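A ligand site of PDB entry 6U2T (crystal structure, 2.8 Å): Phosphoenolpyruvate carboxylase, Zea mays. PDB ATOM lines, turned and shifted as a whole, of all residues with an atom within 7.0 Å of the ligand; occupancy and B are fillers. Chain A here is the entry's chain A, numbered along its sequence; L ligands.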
ATOM      1  N   ASN A 110       6.009  11.313  -2.310  1.00  0.00           N
ATOM      2  CA  ASN A 110       5.049  12.124  -1.580  1.00  0.00           C
ATOM      3  C   ASN A 110       3.626  11.646  -1.836  1.00  0.00           C
ATOM      4  O   ASN A 110       2.779  11.688  -0.934  1.00  0.00           O
ATOM      5  CB  ASN A 110       5.199  13.597  -1.953  1.00  0.00           C
ATOM      6  CG  ASN A 110       6.336  14.272  -1.227  1.00  0.00           C
ATOM      7  OD1 ASN A 110       7.233  14.851  -1.835  1.00  0.00           O
ATOM      8  ND2 ASN A 110       6.304  14.213   0.106  1.00  0.00           N
ATOM      9  N   GLU A 113       3.119   8.669   0.305  1.00  0.00           N
ATOM     10  CA  GLU A 113       2.926   9.155   1.665  1.00  0.00           C
ATOM     11  C   GLU A 113       1.498   9.650   1.862  1.00  0.00           C
ATOM     12  O   GLU A 113       0.895   9.423   2.925  1.00  0.00           O
ATOM     13  CB  GLU A 113       3.923  10.274   1.961  1.00  0.00           C
ATOM     14  CG  GLU A 113       4.144  10.534   3.446  1.00  0.00           C
ATOM     15  CD  GLU A 113       5.104  11.685   3.692  1.00  0.00           C
ATOM     16  OE1 GLU A 113       5.980  11.922   2.824  1.00  0.00           O
ATOM     17  OE2 GLU A 113       4.987  12.364   4.746  1.00  0.00           O
ATOM     18  N   ILE A 117      -1.356   8.007   4.511  1.00  0.00           N
ATOM     19  CA  ILE A 117      -2.035   8.793   5.544  1.00  0.00           C
ATOM     20  C   ILE A 117      -3.543   8.682   5.374  1.00  0.00           C
ATOM     21  O   ILE A 117      -4.284   8.506   6.341  1.00  0.00           O
ATOM     22  CB  ILE A 117      -1.588  10.261   5.488  1.00  0.00           C
ATOM     23  CG1 ILE A 117      -0.087  10.390   5.743  1.00  0.00           C
ATOM     24  CG2 ILE A 117      -2.355  11.086   6.514  1.00  0.00           C
ATOM     25  CD1 ILE A 117       0.464  11.750   5.342  1.00  0.00           C
ATOM     26  N   GLY A 643       3.928  29.365  11.307  1.00  0.00           N
ATOM     27  CA  GLY A 643       3.477  29.144  12.660  1.00  0.00           C
ATOM     28  C   GLY A 643       3.308  27.677  13.003  1.00  0.00           C
ATOM     29  O   GLY A 643       3.409  26.787  12.156  1.00  0.00           O
ATOM     30  N   THR A 644       3.058  27.439  14.291  1.00  0.00           N
ATOM     31  CA  THR A 644       2.652  26.106  14.707  1.00  0.00           C
ATOM     32  C   THR A 644       1.262  25.789  14.197  1.00  0.00           C
ATOM     33  O   THR A 644       1.018  24.711  13.643  1.00  0.00           O
ATOM     34  CB  THR A 644       2.728  26.011  16.230  1.00  0.00           C
ATOM     35  OG1 THR A 644       1.866  26.993  16.809  1.00  0.00           O
ATOM     36  CG2 THR A 644       4.148  26.251  16.699  1.00  0.00           C
ATOM     37  N   GLY A 646      -1.192  25.993  11.329  1.00  0.00           N
ATOM     38  CA  GLY A 646      -0.835  26.004   9.930  1.00  0.00           C
ATOM     39  C   GLY A 646       0.202  24.981   9.537  1.00  0.00           C
ATOM     40  O   GLY A 646       0.579  24.918   8.354  1.00  0.00           O
ATOM     41  N   ARG A 647       0.710  24.192  10.487  1.00  0.00           N
ATOM     42  CA  ARG A 647       1.496  23.021  10.144  1.00  0.00           C
ATOM     43  C   ARG A 647       0.618  21.978   9.461  1.00  0.00           C
ATOM     44  O   ARG A 647      -0.603  21.990   9.574  1.00  0.00           O
ATOM     45  CB  ARG A 647       2.143  22.417  11.400  1.00  0.00           C
ATOM     46  CG  ARG A 647       3.380  23.138  11.888  1.00  0.00           C
ATOM     47  CD  ARG A 647       3.984  22.448  13.109  1.00  0.00           C
ATOM     48  NE  ARG A 647       4.477  21.106  12.791  1.00  0.00           N
ATOM     49  CZ  ARG A 647       4.947  20.249  13.694  1.00  0.00           C
ATOM     50  NH1 ARG A 647       4.980  20.581  14.979  1.00  0.00           N
ATOM     51  NH2 ARG A 647       5.385  19.059  13.312  1.00  0.00           N
ATOM     52  N   GLY A 648       1.264  21.063   8.740  1.00  0.00           N
ATOM     53  CA  GLY A 648       0.533  20.034   8.026  1.00  0.00           C
ATOM     54  C   GLY A 648       0.127  18.902   8.957  1.00  0.00           C
ATOM     55  O   GLY A 648       0.961  18.370   9.698  1.00  0.00           O
ATOM     56  N   GLY A 649      -1.153  18.537   8.922  1.00  0.00           N
ATOM     57  CA  GLY A 649      -1.599  17.374   9.650  1.00  0.00           C
ATOM     58  C   GLY A 649      -1.908  17.665  11.110  1.00  0.00           C
ATOM     59  O   GLY A 649      -2.223  18.793  11.495  1.00  0.00           O
ATOM     60  N   GLY A 650      -1.774  16.620  11.941  1.00  0.00           N
ATOM     61  CA  GLY A 650      -2.145  16.707  13.335  1.00  0.00           C
ATOM     62  C   GLY A 650      -1.587  17.865  14.143  1.00  0.00           C
ATOM     63  O   GLY A 650      -2.310  18.405  14.984  1.00  0.00           O
ATOM     64  N   PRO A 651      -0.319  18.240  13.967  1.00  0.00           N
ATOM     65  CA  PRO A 651       0.247  19.312  14.813  1.00  0.00           C
ATOM     66  C   PRO A 651      -0.594  20.573  14.914  1.00  0.00           C
ATOM     67  O   PRO A 651      -0.583  21.238  15.956  1.00  0.00           O
ATOM     68  CB  PRO A 651       1.603  19.601  14.150  1.00  0.00           C
ATOM     69  CG  PRO A 651       2.007  18.311  13.578  1.00  0.00           C
ATOM     70  CD  PRO A 651       0.737  17.608  13.139  1.00  0.00           C
ATOM     71  N   THR A 652      -1.335  20.929  13.856  1.00  0.00           N
ATOM     72  CA  THR A 652      -2.201  22.094  13.916  1.00  0.00           C
ATOM     73  C   THR A 652      -3.309  21.928  14.948  1.00  0.00           C
ATOM     74  O   THR A 652      -3.677  22.892  15.635  1.00  0.00           O
ATOM     75  CB  THR A 652      -2.789  22.382  12.527  1.00  0.00           C
ATOM     76  OG1 THR A 652      -1.816  23.086  11.735  1.00  0.00           O
ATOM     77  CG2 THR A 652      -4.043  23.238  12.627  1.00  0.00           C
ATOM     78  N   GLU A 675       3.415  25.565   0.925  1.00  0.00           N
ATOM     79  CA  GLU A 675       4.288  24.419   1.121  1.00  0.00           C
ATOM     80  C   GLU A 675       3.538  23.214   1.671  1.00  0.00           C
ATOM     81  O   GLU A 675       3.979  22.065   1.474  1.00  0.00           O
ATOM     82  CB  GLU A 675       5.437  24.788   2.062  1.00  0.00           C
ATOM     83  CG  GLU A 675       6.313  25.932   1.552  1.00  0.00           C
ATOM     84  CD  GLU A 675       6.086  27.231   2.319  1.00  0.00           C
ATOM     85  OE1 GLU A 675       6.264  28.314   1.725  1.00  0.00           O
ATOM     86  OE2 GLU A 675       5.749  27.143   3.519  1.00  0.00           O
ATOM     87  N   VAL A 676       2.412  23.426   2.345  1.00  0.00           N
ATOM     88  CA  VAL A 676       1.638  22.335   2.937  1.00  0.00           C
ATOM     89  C   VAL A 676       0.276  22.144   2.271  1.00  0.00           C
ATOM     90  O   VAL A 676      -0.468  21.251   2.683  1.00  0.00           O
ATOM     91  CB  VAL A 676       1.450  22.542   4.458  1.00  0.00           C
ATOM     92  CG1 VAL A 676       2.785  22.715   5.137  1.00  0.00           C
ATOM     93  CG2 VAL A 676       0.530  23.730   4.730  1.00  0.00           C
ATOM     94  N   PHE A 679      -0.505  18.523   0.864  1.00  0.00           N
ATOM     95  CA  PHE A 679      -0.775  17.517   1.879  1.00  0.00           C
ATOM     96  C   PHE A 679      -2.072  17.799   2.630  1.00  0.00           C
ATOM     97  O   PHE A 679      -2.657  16.862   3.190  1.00  0.00           O
ATOM     98  CB  PHE A 679       0.391  17.424   2.865  1.00  0.00           C
ATOM     99  CG  PHE A 679       1.401  16.372   2.502  1.00  0.00           C
ATOM    100  CD1 PHE A 679       1.997  16.374   1.260  1.00  0.00           C
ATOM    101  CD2 PHE A 679       1.735  15.372   3.408  1.00  0.00           C
ATOM    102  CE1 PHE A 679       2.927  15.411   0.912  1.00  0.00           C
ATOM    103  CE2 PHE A 679       2.660  14.397   3.063  1.00  0.00           C
ATOM    104  CZ  PHE A 679       3.252  14.416   1.821  1.00  0.00           C
ATOM    105  N   CYS A 680      -2.528  19.048   2.652  1.00  0.00           N
ATOM    106  CA  CYS A 680      -3.728  19.387   3.404  1.00  0.00           C
ATOM    107  C   CYS A 680      -4.988  19.185   2.581  1.00  0.00           C
ATOM    108  O   CYS A 680      -6.021  18.769   3.112  1.00  0.00           O
ATOM    109  CB  CYS A 680      -3.654  20.828   3.909  1.00  0.00           C
ATOM    110  SG  CYS A 680      -2.403  21.132   5.192  1.00  0.00           S
ATOM    111  N   LEU A 828       7.770  21.874  17.012  1.00  0.00           N
ATOM    112  CA  LEU A 828       8.149  22.520  15.771  1.00  0.00           C
ATOM    113  C   LEU A 828       9.655  22.414  15.536  1.00  0.00           C
ATOM    114  O   LEU A 828      10.099  22.066  14.434  1.00  0.00           O
ATOM    115  CB  LEU A 828       7.711  23.991  15.776  1.00  0.00           C
ATOM    116  CG  LEU A 828       7.807  24.744  14.446  1.00  0.00           C
ATOM    117  CD1 LEU A 828       6.476  25.335  14.062  1.00  0.00           C
ATOM    118  CD2 LEU A 828       8.871  25.831  14.511  1.00  0.00           C
ATOM    119  N   MET A 831      10.673  18.808  14.591  1.00  0.00           N
ATOM    120  CA  MET A 831      10.375  18.486  13.198  1.00  0.00           C
ATOM    121  C   MET A 831      11.402  19.098  12.256  1.00  0.00           C
ATOM    122  O   MET A 831      11.827  18.465  11.286  1.00  0.00           O
ATOM    123  CB  MET A 831       8.972  18.956  12.842  1.00  0.00           C
ATOM    124  CG  MET A 831       8.537  18.638  11.420  1.00  0.00           C
ATOM    125  SD  MET A 831       8.861  20.001  10.273  1.00  0.00           S
ATOM    126  CE  MET A 831       7.726  21.238  10.889  1.00  0.00           C
ATOM    127  N   LYS A 835      14.432  17.396   9.606  1.00  0.00           N
ATOM    128  CA  LYS A 835      14.645  17.813   8.236  1.00  0.00           C
ATOM    129  C   LYS A 835      16.022  18.413   8.005  1.00  0.00           C
ATOM    130  O   LYS A 835      16.364  18.715   6.856  1.00  0.00           O
ATOM    131  CB  LYS A 835      13.560  18.813   7.836  1.00  0.00           C
ATOM    132  CG  LYS A 835      12.144  18.279   7.906  1.00  0.00           C
ATOM    133  CD  LYS A 835      11.161  19.329   7.429  1.00  0.00           C
ATOM    134  CE  LYS A 835       9.818  18.719   7.117  1.00  0.00           C
ATOM    135  NZ  LYS A 835       8.803  19.760   6.792  1.00  0.00           N
ATOM    136  N   ASP A 884       6.845  10.657  17.589  1.00  0.00           N
ATOM    137  CA  ASP A 884       5.989  10.518  16.410  1.00  0.00           C
ATOM    138  C   ASP A 884       6.709   9.677  15.374  1.00  0.00           C
ATOM    139  O   ASP A 884       7.306  10.200  14.419  1.00  0.00           O
ATOM    140  CB  ASP A 884       5.607  11.900  15.842  1.00  0.00           C
ATOM    141  CG  ASP A 884       4.411  11.840  14.909  1.00  0.00           C
ATOM    142  OD1 ASP A 884       4.259  10.837  14.186  1.00  0.00           O
ATOM    143  OD2 ASP A 884       3.617  12.812  14.908  1.00  0.00           O
ATOM    144  N   LEU A 887       5.563  10.373  11.632  1.00  0.00           N
ATOM    145  CA  LEU A 887       6.189  11.531  10.992  1.00  0.00           C
ATOM    146  C   LEU A 887       7.652  11.272  10.678  1.00  0.00           C
ATOM    147  O   LEU A 887       8.155  11.653   9.615  1.00  0.00           O
ATOM    148  CB  LEU A 887       6.034  12.771  11.875  1.00  0.00           C
ATOM    149  CG  LEU A 887       6.617  14.087  11.358  1.00  0.00           C
ATOM    150  CD1 LEU A 887       5.984  14.473  10.037  1.00  0.00           C
ATOM    151  CD2 LEU A 887       6.437  15.189  12.390  1.00  0.00           C
ATOM    152  N   GLY A 890       7.885   9.163   7.541  1.00  0.00           N
ATOM    153  CA  GLY A 890       7.536   9.904   6.349  1.00  0.00           C
ATOM    154  C   GLY A 890       8.599  10.903   5.940  1.00  0.00           C
ATOM    155  O   GLY A 890       8.908  11.044   4.753  1.00  0.00           O
ATOM    156  N   LEU A 891       9.199  11.584   6.916  1.00  0.00           N
ATOM    157  CA  LEU A 891      10.239  12.549   6.582  1.00  0.00           C
ATOM    158  C   LEU A 891      11.484  11.842   6.061  1.00  0.00           C
ATOM    159  O   LEU A 891      12.056  12.275   5.057  1.00  0.00           O
ATOM    160  CB  LEU A 891      10.565  13.400   7.804  1.00  0.00           C
ATOM    161  CG  LEU A 891       9.425  14.314   8.282  1.00  0.00           C
ATOM    162  CD1 LEU A 891       9.892  15.142   9.472  1.00  0.00           C
ATOM    163  CD2 LEU A 891       8.934  15.197   7.154  1.00  0.00           C
ATOM    164  N   ARG A 894      11.931  10.707   2.351  1.00  0.00           N
ATOM    165  CA  ARG A 894      12.120  11.724   1.322  1.00  0.00           C
ATOM    166  C   ARG A 894      13.594  12.054   1.098  1.00  0.00           C
ATOM    167  O   ARG A 894      13.966  12.483  -0.001  1.00  0.00           O
ATOM    168  CB  ARG A 894      11.386  13.013   1.684  1.00  0.00           C
ATOM    169  CG  ARG A 894       9.919  12.882   2.021  1.00  0.00           C
ATOM    170  CD  ARG A 894       9.375  14.227   2.452  1.00  0.00           C
ATOM    171  NE  ARG A 894       8.042  14.131   3.053  1.00  0.00           N
ATOM    172  CZ  ARG A 894       7.460  15.113   3.733  1.00  0.00           C
ATOM    173  NH1 ARG A 894       8.071  16.268   3.906  1.00  0.00           N
ATOM    174  NH2 ARG A 894       6.239  14.927   4.245  1.00  0.00           N
ATOM    175  N   ALA A 964      10.165  21.214  -2.338  1.00  0.00           N
ATOM    176  CA  ALA A 964       9.098  20.223  -2.312  1.00  0.00           C
ATOM    177  C   ALA A 964       9.322  19.204  -1.198  1.00  0.00           C
ATOM    178  O   ALA A 964       8.369  18.798  -0.518  1.00  0.00           O
ATOM    179  CB  ALA A 964       8.995  19.524  -3.666  1.00  0.00           C
ATOM    180  N   GLY A 965      10.570  18.786  -0.985  1.00  0.00           N
ATOM    181  CA  GLY A 965      10.846  17.812   0.049  1.00  0.00           C
ATOM    182  C   GLY A 965      10.802  18.385   1.454  1.00  0.00           C
ATOM    183  O   GLY A 965      10.418  17.701   2.402  1.00  0.00           O
ATOM    184  N   MET A 966      11.180  19.654   1.602  1.00  0.00           N
ATOM    185  CA  MET A 966      11.277  20.262   2.930  1.00  0.00           C
ATOM    186  C   MET A 966       9.961  20.835   3.433  1.00  0.00           C
ATOM    187  O   MET A 966       9.781  20.919   4.649  1.00  0.00           O
ATOM    188  CB  MET A 966      12.338  21.370   2.924  1.00  0.00           C
ATOM    189  CG  MET A 966      13.722  20.896   2.512  1.00  0.00           C
ATOM    190  SD  MET A 966      14.350  19.574   3.565  1.00  0.00           S
ATOM    191  CE  MET A 966      14.494  20.498   5.060  1.00  0.00           C
ATOM    192  N   GLN A 967       9.061  21.226   2.535  1.00  0.00           N
ATOM    193  CA  GLN A 967       7.719  21.749   2.870  1.00  0.00           C
ATOM    194  C   GLN A 967       7.873  22.853   3.919  1.00  0.00           C
ATOM    195  O   GLN A 967       8.679  23.777   3.709  1.00  0.00           O
ATOM    196  CB  GLN A 967       6.810  20.594   3.265  1.00  0.00           C
ATOM    197  CG  GLN A 967       6.425  19.667   2.113  1.00  0.00           C
ATOM    198  CD  GLN A 967       5.339  18.680   2.507  1.00  0.00           C
ATOM    199  OE1 GLN A 967       5.498  17.459   2.365  1.00  0.00           O
ATOM    200  NE2 GLN A 967       4.237  19.201   3.029  1.00  0.00           N
ATOM    201  N   ASN A 968       7.160  22.793   5.039  1.00  0.00           N
ATOM    202  CA  ASN A 968       7.160  23.869   6.023  1.00  0.00           C
ATOM    203  C   ASN A 968       8.283  23.690   7.036  1.00  0.00           C
ATOM    204  O   ASN A 968       8.457  22.594   7.588  1.00  0.00           O
ATOM    205  CB  ASN A 968       5.815  23.927   6.743  1.00  0.00           C
ATOM    206  CG  ASN A 968       5.445  22.607   7.373  1.00  0.00           C
ATOM    207  OD1 ASN A 968       5.547  21.567   6.727  1.00  0.00           O
ATOM    208  ND2 ASN A 968       5.036  22.640   8.634  1.00  0.00           N
HETATM  209  C1  LIG L   1       4.484  19.104   9.758  1.00  0.00           C
HETATM  210  O1  LIG L   1       4.180  20.208  10.272  1.00  0.00           O
HETATM  211  O2  LIG L   1       4.422  18.066  10.454  1.00  0.00           O
HETATM  212  C2  LIG L   1       4.944  19.030   8.335  1.00  0.00           C
HETATM  213  O3  LIG L   1       3.864  19.358   7.472  1.00  0.00           O
HETATM  214  C3  LIG L   1       5.475  17.638   8.029  1.00  0.00           C
HETATM  215  C4  LIG L   1       5.850  17.515   6.562  1.00  0.00           C
HETATM  216  O4  LIG L   1       6.747  18.233   6.061  1.00  0.00           O
HETATM  217  O5  LIG L   1       5.275  16.680   5.831  1.00  0.00           O
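OE1 of Gln 967 is in hydrogen-bond range of NH1 of Arg 894 (3.2 Å).
The guanidinium group (NH2) of Arg 894 lies within salt-bridge range of the side-chain carboxylate (OE2) of Glu 113, 2.9 Å away.
The backbone carbonyl oxygen (O) of Gly 965 sits at hydrogen-bond distance from the guanidinium group (NH1) of Arg 894, at 3.1 Å.
NE of Arg 894 sits close to ND2 of Asn 110, at 3.4 Å.
The backbone carbonyl oxygen (O) of Asn 968 sits at hydrogen-bond distance from the side-chain amino group (NZ) of Lys 835 (3.0 Å).
The backbone carbonyl oxygen (O) of Met 966 is in hydrogen-bond range of the side-chain amino group (NZ) of Lys 835 (2.6 Å).
O of Arg 647 is in hydrogen-bond range of OG1 of Thr 652.
The side-chain carboxylate (OD1) of Asp 884 is in hydrogen-bond range of the backbone NH (N) of Leu 887 (2.9 Å).
The guanidinium group of Arg 894 lies within salt-bridge range of an oxygen (O5) of the ligand (2.6 Å).
The side-chain amino group of Lys 835 is in salt-bridge range of an oxygen (O4) of the ligand (2.7 Å).
The guanidinium group of Arg 647 lies within salt-bridge range of an oxygen (O1) of the ligand, at 2.7 Å.
An oxygen (O3) of the ligand sits at hydrogen-bond distance from the side-chain amide oxygen (OD1) of Asn 968, 2.9 Å away.
The backbone NH (N) of Gly 648 lies within hydrogen-bond range of an oxygen (O3) of the ligand (3.4 Å).
Pro 651 touches the ligand.
Met 831 touches the ligand.
Leu 887 touches the ligand.
Leu 891 touches the ligand (CD2 to O4, 3.9 Å).
Gln 967 touches the ligand.
Hydrophobic or aromatic side chains that line the ligand: Pro 651, Met 831, Leu 887 and Leu 891.
Of the 29 residues printed, 10 come within 4 Å of the ligand.
The nearest printed residue that does not touch the ligand is Val 676 (4.2 Å).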
